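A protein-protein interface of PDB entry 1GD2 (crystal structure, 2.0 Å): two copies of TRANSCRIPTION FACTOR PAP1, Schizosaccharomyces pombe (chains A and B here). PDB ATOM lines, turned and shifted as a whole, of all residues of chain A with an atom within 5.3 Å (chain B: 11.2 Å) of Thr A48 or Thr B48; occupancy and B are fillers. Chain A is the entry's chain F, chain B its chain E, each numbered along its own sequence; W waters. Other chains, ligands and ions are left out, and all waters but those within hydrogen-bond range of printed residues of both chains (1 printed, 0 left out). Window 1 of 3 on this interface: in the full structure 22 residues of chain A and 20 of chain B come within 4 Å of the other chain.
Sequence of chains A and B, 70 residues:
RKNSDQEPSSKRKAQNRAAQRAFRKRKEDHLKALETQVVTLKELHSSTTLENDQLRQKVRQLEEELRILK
Water W1 lies within hydrogen-bond range of OG1 of Thr A48 (2.8 Å), ND1 of His B45 (3.0 Å), O of Leu A44 (3.1 Å), OG1 of Thr B48 (3.4 Å) and N of His A45 (3.4 Å).
Leu A44 touches His B45, and with the chains exchanged His A45 touches Leu B44.
His A45 touches Thr B48, but with the chains exchanged Thr A48 does not touch His B45 (4.7 Å).
Asn A52 touches Thr B48, but with the chains exchanged Thr A48 does not touch Asn B52 (4.7 Å).
Asn B52 touches its own counterpart, Asn A52.
His B45 touches Leu A44 (CE1 to CD1, 3.7 Å).
NE2 of His A45 touches CD2 of Leu B44 (3.5 Å).
Thr B48 touches His A45.
Thr A49 touches Thr B48.
Leu B55 touches Asn A52.
OE2 of Glu A51 lies within hydrogen-bond range of ND2 of Asn B52 (2.9 Å).
The backbone carbonyl oxygen (O) of Thr B48 lies within hydrogen-bond range of the side-chain amide nitrogen (ND2) of Asn A52, 3.1 Å away.
OG1 of Thr B48 lies within hydrogen-bond range of OG1 of Thr A48.
The side-chain amide nitrogen of Asn A52 lies within hydrogen-bond range of the side-chain carboxylate of Glu B51 (3.2 Å).
ND2 of Asn B52 lies close to OD1 of Asn A52 (3.4 Å).
The guanidinium group of Arg B56 lies within salt-bridge range of the side-chain carboxylate of Glu A51 (2.8 Å).
Of the 10 printed residues of chain A, 6 touch a printed residue of chain B.
Printed residues of chain A that touch a printed residue of chain B: Leu A44, His A45, Thr A48, Thr A49, Glu A51 and Asn A52.
Hydrophobic or aromatic side chains of chain A within 4 Å of the printed part of chain B: Leu A44 and His A45.
Of the 18 printed residues of chain B, 7 touch a printed residue of chain A.
Printed residues of chain B that touch a printed residue of chain A: Leu B44, His B45, Thr B48, Glu B51, Asn B52, Leu B55 and Arg B56.
Among the printed residues, 11 pairs touch across the chains.
Among the printed residues, Asp or Glu carboxylates within 4 Å of a Lys or Arg side-chain nitrogen of the other chain: Glu A51 with Arg B56 (2.8 Å).
NH1 of Arg B56 lies within hydrogen-bond range of OD1 of Asn B52, 3.0 Å away.
The backbone carbonyl oxygen (O) of Leu A44 sits at hydrogen-bond distance from the side-chain hydroxyl (OG) of Ser A47 (3.2 Å).
The backbone carbonyl oxygen (O) of His A45 sits at hydrogen-bond distance from the side-chain hydroxyl (OG1) of Thr A49, 3.0 Å away.
The backbone carbonyl oxygen of Thr A48 lies close to the side-chain amide oxygen of Asn A52, 3.1 Å away.
The backbone carbonyl oxygen (O) of Leu B44 sits at hydrogen-bond distance from the side-chain hydroxyl (OG1) of Thr B48, at 2.9 Å.
OG1 of Thr B49 lies within hydrogen-bond range of O of His B45, at 2.7 Å.
Thr A48 touches one residue of chain B.
Of the printed residues of chain A, Thr B48 touches His A45, Thr A48, Thr A49 and Asn A52.
Leu A44 touches just one residue of chain B: His B45 (3.7 Å).
No residue of chain B comes within 4 Å of Ser A46.
Ser A47 touches none of the printed residues of chain B.
Of chain B, only Thr B48 comes within 4 Å of Thr A49.
Asn A52 touches just these residues of chain B: Thr B48 (3.1 Å), Glu B51 (3.2 Å), Asn B52 (3.3 Å) and Leu B55 (3.6 Å).
Of the printed residues of chain A, Arg B56 touches Glu A51.
Printed residues of chain A within 4 Å of Asn B52: Glu A51 and Asn A52.
Asp B53 touches none of the printed residues of chain A.
Ser B47 touches none of the printed residues of chain A.
The nearest printed residue of chain B that does not touch Thr A48 is Asn B52 (4.7 Å).
The nearest printed residue of chain A that does not touch Leu B55 is Glu A51 (5.3 Å).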
ATOM      1  N   GLU A  43     -21.762  23.464 -35.961  1.00  0.00           N
ATOM      2  CA  GLU A  43     -22.954  22.688 -36.301  1.00  0.00           C
ATOM      3  C   GLU A  43     -23.189  21.721 -35.142  1.00  0.00           C
ATOM      4  O   GLU A  43     -24.329  21.431 -34.779  1.00  0.00           O
ATOM      5  CB  GLU A  43     -22.736  21.897 -37.598  1.00  0.00           C
ATOM      6  CG  GLU A  43     -22.447  22.771 -38.818  1.00  0.00           C
ATOM      7  CD  GLU A  43     -21.996  21.983 -40.045  1.00  0.00           C
ATOM      8  OE1 GLU A  43     -21.637  20.791 -39.920  1.00  0.00           O
ATOM      9  OE2 GLU A  43     -21.986  22.572 -41.146  1.00  0.00           O
ATOM     10  N   LEU A  44     -22.089  21.249 -34.556  1.00  0.00           N
ATOM     11  CA  LEU A  44     -22.114  20.325 -33.430  1.00  0.00           C
ATOM     12  C   LEU A  44     -22.670  21.009 -32.187  1.00  0.00           C
ATOM     13  O   LEU A  44     -23.365  20.383 -31.388  1.00  0.00           O
ATOM     14  CB  LEU A  44     -20.700  19.821 -33.131  1.00  0.00           C
ATOM     15  CG  LEU A  44     -20.447  18.317 -33.161  1.00  0.00           C
ATOM     16  CD1 LEU A  44     -19.024  18.054 -32.725  1.00  0.00           C
ATOM     17  CD2 LEU A  44     -21.415  17.598 -32.242  1.00  0.00           C
ATOM     18  N   HIS A  45     -22.339  22.286 -32.015  1.00  0.00           N
ATOM     19  CA  HIS A  45     -22.809  23.052 -30.867  1.00  0.00           C
ATOM     20  C   HIS A  45     -24.283  23.421 -30.991  1.00  0.00           C
ATOM     21  O   HIS A  45     -25.031  23.375 -30.017  1.00  0.00           O
ATOM     22  CB  HIS A  45     -21.988  24.326 -30.691  1.00  0.00           C
ATOM     23  CG  HIS A  45     -22.451  25.175 -29.551  1.00  0.00           C
ATOM     24  ND1 HIS A  45     -22.579  24.687 -28.268  1.00  0.00           N
ATOM     25  CD2 HIS A  45     -22.859  26.464 -29.507  1.00  0.00           C
ATOM     26  CE1 HIS A  45     -23.051  25.639 -27.483  1.00  0.00           C
ATOM     27  NE2 HIS A  45     -23.229  26.727 -28.210  1.00  0.00           N
ATOM     28  N   SER A  46     -24.679  23.802 -32.201  1.00  0.00           N
ATOM     29  CA  SER A  46     -26.052  24.192 -32.504  1.00  0.00           C
ATOM     30  C   SER A  46     -27.037  23.019 -32.370  1.00  0.00           C
ATOM     31  O   SER A  46     -28.224  23.227 -32.103  1.00  0.00           O
ATOM     32  CB  SER A  46     -26.108  24.776 -33.922  1.00  0.00           C
ATOM     33  OG  SER A  46     -27.334  25.438 -34.175  1.00  0.00           O
ATOM     34  N   SER A  47     -26.535  21.793 -32.532  1.00  0.00           N
ATOM     35  CA  SER A  47     -27.367  20.594 -32.446  1.00  0.00           C
ATOM     36  C   SER A  47     -27.456  19.998 -31.045  1.00  0.00           C
ATOM     37  O   SER A  47     -28.513  19.503 -30.656  1.00  0.00           O
ATOM     38  CB  SER A  47     -26.895  19.523 -33.438  1.00  0.00           C
ATOM     39  OG  SER A  47     -25.724  18.865 -32.985  1.00  0.00           O
ATOM     40  N   THR A  48     -26.350  20.006 -30.301  1.00  0.00           N
ATOM     41  CA  THR A  48     -26.359  19.461 -28.942  1.00  0.00           C
ATOM     42  C   THR A  48     -27.093  20.410 -28.000  1.00  0.00           C
ATOM     43  O   THR A  48     -27.646  19.981 -26.989  1.00  0.00           O
ATOM     44  CB  THR A  48     -24.937  19.188 -28.390  1.00  0.00           C
ATOM     45  OG1 THR A  48     -24.186  20.407 -28.365  1.00  0.00           O
ATOM     46  CG2 THR A  48     -24.210  18.154 -29.245  1.00  0.00           C
ATOM     47  N   THR A  49     -27.098  21.696 -28.347  1.00  0.00           N
ATOM     48  CA  THR A  49     -27.783  22.712 -27.554  1.00  0.00           C
ATOM     49  C   THR A  49     -29.290  22.669 -27.839  1.00  0.00           C
ATOM     50  O   THR A  49     -30.096  23.074 -27.001  1.00  0.00           O
ATOM     51  CB  THR A  49     -27.197  24.127 -27.814  1.00  0.00           C
ATOM     52  OG1 THR A  49     -25.862  24.187 -27.295  1.00  0.00           O
ATOM     53  CG2 THR A  49     -28.030  25.205 -27.132  1.00  0.00           C
ATOM     54  N   LEU A  50     -29.665  22.163 -29.012  1.00  0.00           N
ATOM     55  CA  LEU A  50     -31.074  22.034 -29.380  1.00  0.00           C
ATOM     56  C   LEU A  50     -31.636  20.801 -28.673  1.00  0.00           C
ATOM     57  O   LEU A  50     -32.816  20.754 -28.320  1.00  0.00           O
ATOM     58  CB  LEU A  50     -31.233  21.875 -30.897  1.00  0.00           C
ATOM     59  CG  LEU A  50     -32.657  21.708 -31.444  1.00  0.00           C
ATOM     60  CD1 LEU A  50     -33.443  23.004 -31.272  1.00  0.00           C
ATOM     61  CD2 LEU A  50     -32.610  21.304 -32.912  1.00  0.00           C
ATOM     62  N   GLU A  51     -30.776  19.803 -28.475  1.00  0.00           N
ATOM     63  CA  GLU A  51     -31.155  18.568 -27.803  1.00  0.00           C
ATOM     64  C   GLU A  51     -31.279  18.818 -26.304  1.00  0.00           C
ATOM     65  O   GLU A  51     -32.010  18.115 -25.608  1.00  0.00           O
ATOM     66  CB  GLU A  51     -30.122  17.473 -28.072  1.00  0.00           C
ATOM     67  CG  GLU A  51     -30.575  16.090 -27.636  1.00  0.00           C
ATOM     68  CD  GLU A  51     -29.578  14.999 -27.977  1.00  0.00           C
ATOM     69  OE1 GLU A  51     -28.990  15.040 -29.080  1.00  0.00           O
ATOM     70  OE2 GLU A  51     -29.391  14.091 -27.140  1.00  0.00           O
ATOM     71  N   ASN A  52     -30.549  19.817 -25.811  1.00  0.00           N
ATOM     72  CA  ASN A  52     -30.593  20.183 -24.402  1.00  0.00           C
ATOM     73  C   ASN A  52     -31.864  20.970 -24.101  1.00  0.00           C
ATOM     74  O   ASN A  52     -32.358  20.946 -22.978  1.00  0.00           O
ATOM     75  CB  ASN A  52     -29.357  20.992 -24.011  1.00  0.00           C
ATOM     76  CG  ASN A  52     -28.102  20.141 -23.926  1.00  0.00           C
ATOM     77  OD1 ASN A  52     -28.136  18.929 -24.160  1.00  0.00           O
ATOM     78  ND2 ASN A  52     -26.984  20.772 -23.586  1.00  0.00           N
ATOM     79  N   VAL B  39     -10.569  26.377 -29.631  1.00  0.00           N
ATOM     80  CA  VAL B  39     -10.433  25.983 -28.229  1.00  0.00           C
ATOM     81  C   VAL B  39     -11.715  26.338 -27.485  1.00  0.00           C
ATOM     82  O   VAL B  39     -12.206  25.559 -26.671  1.00  0.00           O
ATOM     83  CB  VAL B  39      -9.212  26.666 -27.559  1.00  0.00           C
ATOM     84  CG1 VAL B  39      -9.334  26.638 -26.035  1.00  0.00           C
ATOM     85  CG2 VAL B  39      -7.937  25.954 -27.981  1.00  0.00           C
ATOM     86  N   THR B  40     -12.253  27.513 -27.787  1.00  0.00           N
ATOM     87  CA  THR B  40     -13.487  27.991 -27.179  1.00  0.00           C
ATOM     88  C   THR B  40     -14.635  27.070 -27.585  1.00  0.00           C
ATOM     89  O   THR B  40     -15.494  26.732 -26.774  1.00  0.00           O
ATOM     90  CB  THR B  40     -13.784  29.443 -27.633  1.00  0.00           C
ATOM     91  OG1 THR B  40     -12.792  30.325 -27.089  1.00  0.00           O
ATOM     92  CG2 THR B  40     -15.168  29.896 -27.185  1.00  0.00           C
ATOM     93  N   LEU B  41     -14.616  26.646 -28.845  1.00  0.00           N
ATOM     94  CA  LEU B  41     -15.633  25.762 -29.392  1.00  0.00           C
ATOM     95  C   LEU B  41     -15.511  24.336 -28.857  1.00  0.00           C
ATOM     96  O   LEU B  41     -16.515  23.706 -28.538  1.00  0.00           O
ATOM     97  CB  LEU B  41     -15.577  25.780 -30.926  1.00  0.00           C
ATOM     98  CG  LEU B  41     -16.726  26.476 -31.670  1.00  0.00           C
ATOM     99  CD1 LEU B  41     -17.155  27.747 -30.958  1.00  0.00           C
ATOM    100  CD2 LEU B  41     -16.301  26.768 -33.097  1.00  0.00           C
ATOM    101  N   LYS B  42     -14.287  23.835 -28.741  1.00  0.00           N
ATOM    102  CA  LYS B  42     -14.072  22.488 -28.232  1.00  0.00           C
ATOM    103  C   LYS B  42     -14.489  22.340 -26.773  1.00  0.00           C
ATOM    104  O   LYS B  42     -15.041  21.308 -26.388  1.00  0.00           O
ATOM    105  CB  LYS B  42     -12.611  22.059 -28.407  1.00  0.00           C
ATOM    106  CG  LYS B  42     -12.286  21.488 -29.780  1.00  0.00           C
ATOM    107  CD  LYS B  42     -10.919  20.821 -29.806  1.00  0.00           C
ATOM    108  CE  LYS B  42     -10.659  20.135 -31.144  1.00  0.00           C
ATOM    109  NZ  LYS B  42      -9.363  19.394 -31.149  1.00  0.00           N
ATOM    110  N   GLU B  43     -14.226  23.367 -25.965  1.00  0.00           N
ATOM    111  CA  GLU B  43     -14.572  23.351 -24.540  1.00  0.00           C
ATOM    112  C   GLU B  43     -16.064  23.557 -24.318  1.00  0.00           C
ATOM    113  O   GLU B  43     -16.610  23.151 -23.291  1.00  0.00           O
ATOM    114  CB  GLU B  43     -13.766  24.405 -23.780  1.00  0.00           C
ATOM    115  CG  GLU B  43     -12.264  24.129 -23.810  1.00  0.00           C
ATOM    116  CD  GLU B  43     -11.432  25.160 -23.066  1.00  0.00           C
ATOM    117  OE1 GLU B  43     -10.307  24.797 -22.647  1.00  0.00           O
ATOM    118  OE2 GLU B  43     -11.885  26.321 -22.914  1.00  0.00           O
ATOM    119  N   LEU B  44     -16.706  24.197 -25.292  1.00  0.00           N
ATOM    120  CA  LEU B  44     -18.137  24.459 -25.265  1.00  0.00           C
ATOM    121  C   LEU B  44     -18.850  23.149 -25.616  1.00  0.00           C
ATOM    122  O   LEU B  44     -19.881  22.819 -25.034  1.00  0.00           O
ATOM    123  CB  LEU B  44     -18.467  25.541 -26.294  1.00  0.00           C
ATOM    124  CG  LEU B  44     -19.844  26.201 -26.306  1.00  0.00           C
ATOM    125  CD1 LEU B  44     -20.107  26.879 -24.973  1.00  0.00           C
ATOM    126  CD2 LEU B  44     -19.902  27.216 -27.435  1.00  0.00           C
ATOM    127  N   HIS B  45     -18.273  22.406 -26.561  1.00  0.00           N
ATOM    128  CA  HIS B  45     -18.796  21.115 -27.011  1.00  0.00           C
ATOM    129  C   HIS B  45     -18.731  20.135 -25.857  1.00  0.00           C
ATOM    130  O   HIS B  45     -19.680  19.405 -25.604  1.00  0.00           O
ATOM    131  CB  HIS B  45     -17.965  20.588 -28.195  1.00  0.00           C
ATOM    132  CG  HIS B  45     -18.245  19.159 -28.566  1.00  0.00           C
ATOM    133  ND1 HIS B  45     -19.512  18.688 -28.840  1.00  0.00           N
ATOM    134  CD2 HIS B  45     -17.410  18.103 -28.730  1.00  0.00           C
ATOM    135  CE1 HIS B  45     -19.445  17.406 -29.157  1.00  0.00           C
ATOM    136  NE2 HIS B  45     -18.181  17.028 -29.098  1.00  0.00           N
ATOM    137  N   SER B  46     -17.605  20.144 -25.153  1.00  0.00           N
ATOM    138  CA  SER B  46     -17.391  19.265 -24.013  1.00  0.00           C
ATOM    139  C   SER B  46     -18.302  19.652 -22.843  1.00  0.00           C
ATOM    140  O   SER B  46     -18.693  18.801 -22.043  1.00  0.00           O
ATOM    141  CB  SER B  46     -15.919  19.326 -23.584  1.00  0.00           C
ATOM    142  OG  SER B  46     -15.624  18.381 -22.567  1.00  0.00           O
ATOM    143  N   SER B  47     -18.654  20.934 -22.771  1.00  0.00           N
ATOM    144  CA  SER B  47     -19.513  21.457 -21.712  1.00  0.00           C
ATOM    145  C   SER B  47     -20.989  21.116 -21.931  1.00  0.00           C
ATOM    146  O   SER B  47     -21.657  20.616 -21.023  1.00  0.00           O
ATOM    147  CB  SER B  47     -19.337  22.974 -21.600  1.00  0.00           C
ATOM    148  OG  SER B  47     -20.044  23.490 -20.490  1.00  0.00           O
ATOM    149  N   THR B  48     -21.494  21.397 -23.129  1.00  0.00           N
ATOM    150  CA  THR B  48     -22.887  21.109 -23.462  1.00  0.00           C
ATOM    151  C   THR B  48     -23.147  19.608 -23.645  1.00  0.00           C
ATOM    152  O   THR B  48     -24.300  19.180 -23.710  1.00  0.00           O
ATOM    153  CB  THR B  48     -23.365  21.899 -24.716  1.00  0.00           C
ATOM    154  OG1 THR B  48     -22.430  21.729 -25.788  1.00  0.00           O
ATOM    155  CG2 THR B  48     -23.508  23.385 -24.399  1.00  0.00           C
ATOM    156  N   THR B  49     -22.075  18.821 -23.745  1.00  0.00           N
ATOM    157  CA  THR B  49     -22.187  17.367 -23.887  1.00  0.00           C
ATOM    158  C   THR B  49     -22.321  16.755 -22.496  1.00  0.00           C
ATOM    159  O   THR B  49     -23.046  15.780 -22.311  1.00  0.00           O
ATOM    160  CB  THR B  49     -20.965  16.750 -24.622  1.00  0.00           C
ATOM    161  OG1 THR B  49     -21.009  17.115 -26.007  1.00  0.00           O
ATOM    162  CG2 THR B  49     -20.966  15.227 -24.515  1.00  0.00           C
ATOM    163  N   LEU B  50     -21.614  17.330 -21.525  1.00  0.00           N
ATOM    164  CA  LEU B  50     -21.677  16.862 -20.144  1.00  0.00           C
ATOM    165  C   LEU B  50     -23.086  17.137 -19.627  1.00  0.00           C
ATOM    166  O   LEU B  50     -23.669  16.317 -18.918  1.00  0.00           O
ATOM    167  CB  LEU B  50     -20.651  17.601 -19.274  1.00  0.00           C
ATOM    168  CG  LEU B  50     -20.630  17.285 -17.772  1.00  0.00           C
ATOM    169  CD1 LEU B  50     -20.314  15.817 -17.546  1.00  0.00           C
ATOM    170  CD2 LEU B  50     -19.609  18.154 -17.065  1.00  0.00           C
ATOM    171  N   GLU B  51     -23.626  18.289 -20.022  1.00  0.00           N
ATOM    172  CA  GLU B  51     -24.966  18.717 -19.635  1.00  0.00           C
ATOM    173  C   GLU B  51     -26.009  17.778 -20.237  1.00  0.00           C
ATOM    174  O   GLU B  51     -26.986  17.422 -19.580  1.00  0.00           O
ATOM    175  CB  GLU B  51     -25.209  20.149 -20.112  1.00  0.00           C
ATOM    176  CG  GLU B  51     -26.486  20.779 -19.583  1.00  0.00           C
ATOM    177  CD  GLU B  51     -26.795  22.107 -20.247  1.00  0.00           C
ATOM    178  OE1 GLU B  51     -25.946  23.025 -20.176  1.00  0.00           O
ATOM    179  OE2 GLU B  51     -27.887  22.229 -20.848  1.00  0.00           O
ATOM    180  N   ASN B  52     -25.792  17.384 -21.489  1.00  0.00           N
ATOM    181  CA  ASN B  52     -26.683  16.465 -22.194  1.00  0.00           C
ATOM    182  C   ASN B  52     -26.691  15.122 -21.467  1.00  0.00           C
ATOM    183  O   ASN B  52     -27.718  14.452 -21.395  1.00  0.00           O
ATOM    184  CB  ASN B  52     -26.201  16.279 -23.638  1.00  0.00           C
ATOM    185  CG  ASN B  52     -26.992  15.222 -24.398  1.00  0.00           C
ATOM    186  OD1 ASN B  52     -26.755  14.020 -24.249  1.00  0.00           O
ATOM    187  ND2 ASN B  52     -27.920  15.671 -25.238  1.00  0.00           N
ATOM    188  N   ASP B  53     -25.537  14.748 -20.918  1.00  0.00           N
ATOM    189  CA  ASP B  53     -25.387  13.494 -20.189  1.00  0.00           C
ATOM    190  C   ASP B  53     -25.979  13.566 -18.791  1.00  0.00           C
ATOM    191  O   ASP B  53     -26.267  12.536 -18.181  1.00  0.00           O
ATOM    192  CB  ASP B  53     -23.913  13.091 -20.115  1.00  0.00           C
ATOM    193  CG  ASP B  53     -23.310  12.822 -21.483  1.00  0.00           C
ATOM    194  OD1 ASP B  53     -22.069  12.901 -21.600  1.00  0.00           O
ATOM    195  OD2 ASP B  53     -24.069  12.534 -22.438  1.00  0.00           O
ATOM    196  N   GLN B  54     -26.129  14.784 -18.277  1.00  0.00           N
ATOM    197  CA  GLN B  54     -26.711  15.000 -16.956  1.00  0.00           C
ATOM    198  C   GLN B  54     -28.233  15.011 -17.081  1.00  0.00           C
ATOM    199  O   GLN B  54     -28.946  14.581 -16.173  1.00  0.00           O
ATOM    200  CB  GLN B  54     -26.212  16.319 -16.361  1.00  0.00           C
ATOM    201  CG  GLN B  54     -24.718  16.326 -16.050  1.00  0.00           C
ATOM    202  CD  GLN B  54     -24.207  17.684 -15.595  1.00  0.00           C
ATOM    203  OE1 GLN B  54     -23.326  17.770 -14.740  1.00  0.00           O
ATOM    204  NE2 GLN B  54     -24.747  18.750 -16.178  1.00  0.00           N
ATOM    205  N   LEU B  55     -28.715  15.500 -18.223  1.00  0.00           N
ATOM    206  CA  LEU B  55     -30.142  15.568 -18.521  1.00  0.00           C
ATOM    207  C   LEU B  55     -30.692  14.198 -18.907  1.00  0.00           C
ATOM    208  O   LEU B  55     -31.891  13.949 -18.776  1.00  0.00           O
ATOM    209  CB  LEU B  55     -30.404  16.566 -19.649  1.00  0.00           C
ATOM    210  CG  LEU B  55     -30.783  18.005 -19.283  1.00  0.00           C
ATOM    211  CD1 LEU B  55     -29.895  18.557 -18.177  1.00  0.00           C
ATOM    212  CD2 LEU B  55     -30.683  18.855 -20.534  1.00  0.00           C
ATOM    213  N   ARG B  56     -29.823  13.329 -19.419  1.00  0.00           N
ATOM    214  CA  ARG B  56     -30.219  11.976 -19.801  1.00  0.00           C
ATOM    215  C   ARG B  56     -30.335  11.087 -18.568  1.00  0.00           C
ATOM    216  O   ARG B  56     -31.022  10.066 -18.592  1.00  0.00           O
ATOM    217  CB  ARG B  56     -29.231  11.373 -20.805  1.00  0.00           C
ATOM    218  CG  ARG B  56     -29.534  11.736 -22.245  1.00  0.00           C
ATOM    219  CD  ARG B  56     -28.632  10.999 -23.211  1.00  0.00           C
ATOM    220  NE  ARG B  56     -29.144  11.093 -24.576  1.00  0.00           N
ATOM    221  CZ  ARG B  56     -28.387  11.256 -25.659  1.00  0.00           C
ATOM    222  NH1 ARG B  56     -27.066  11.346 -25.552  1.00  0.00           N
ATOM    223  NH2 ARG B  56     -28.954  11.325 -26.857  1.00  0.00           N
HETATM  224  O   HOH W   1     -21.511  20.946 -28.958  1.00  0.00           O
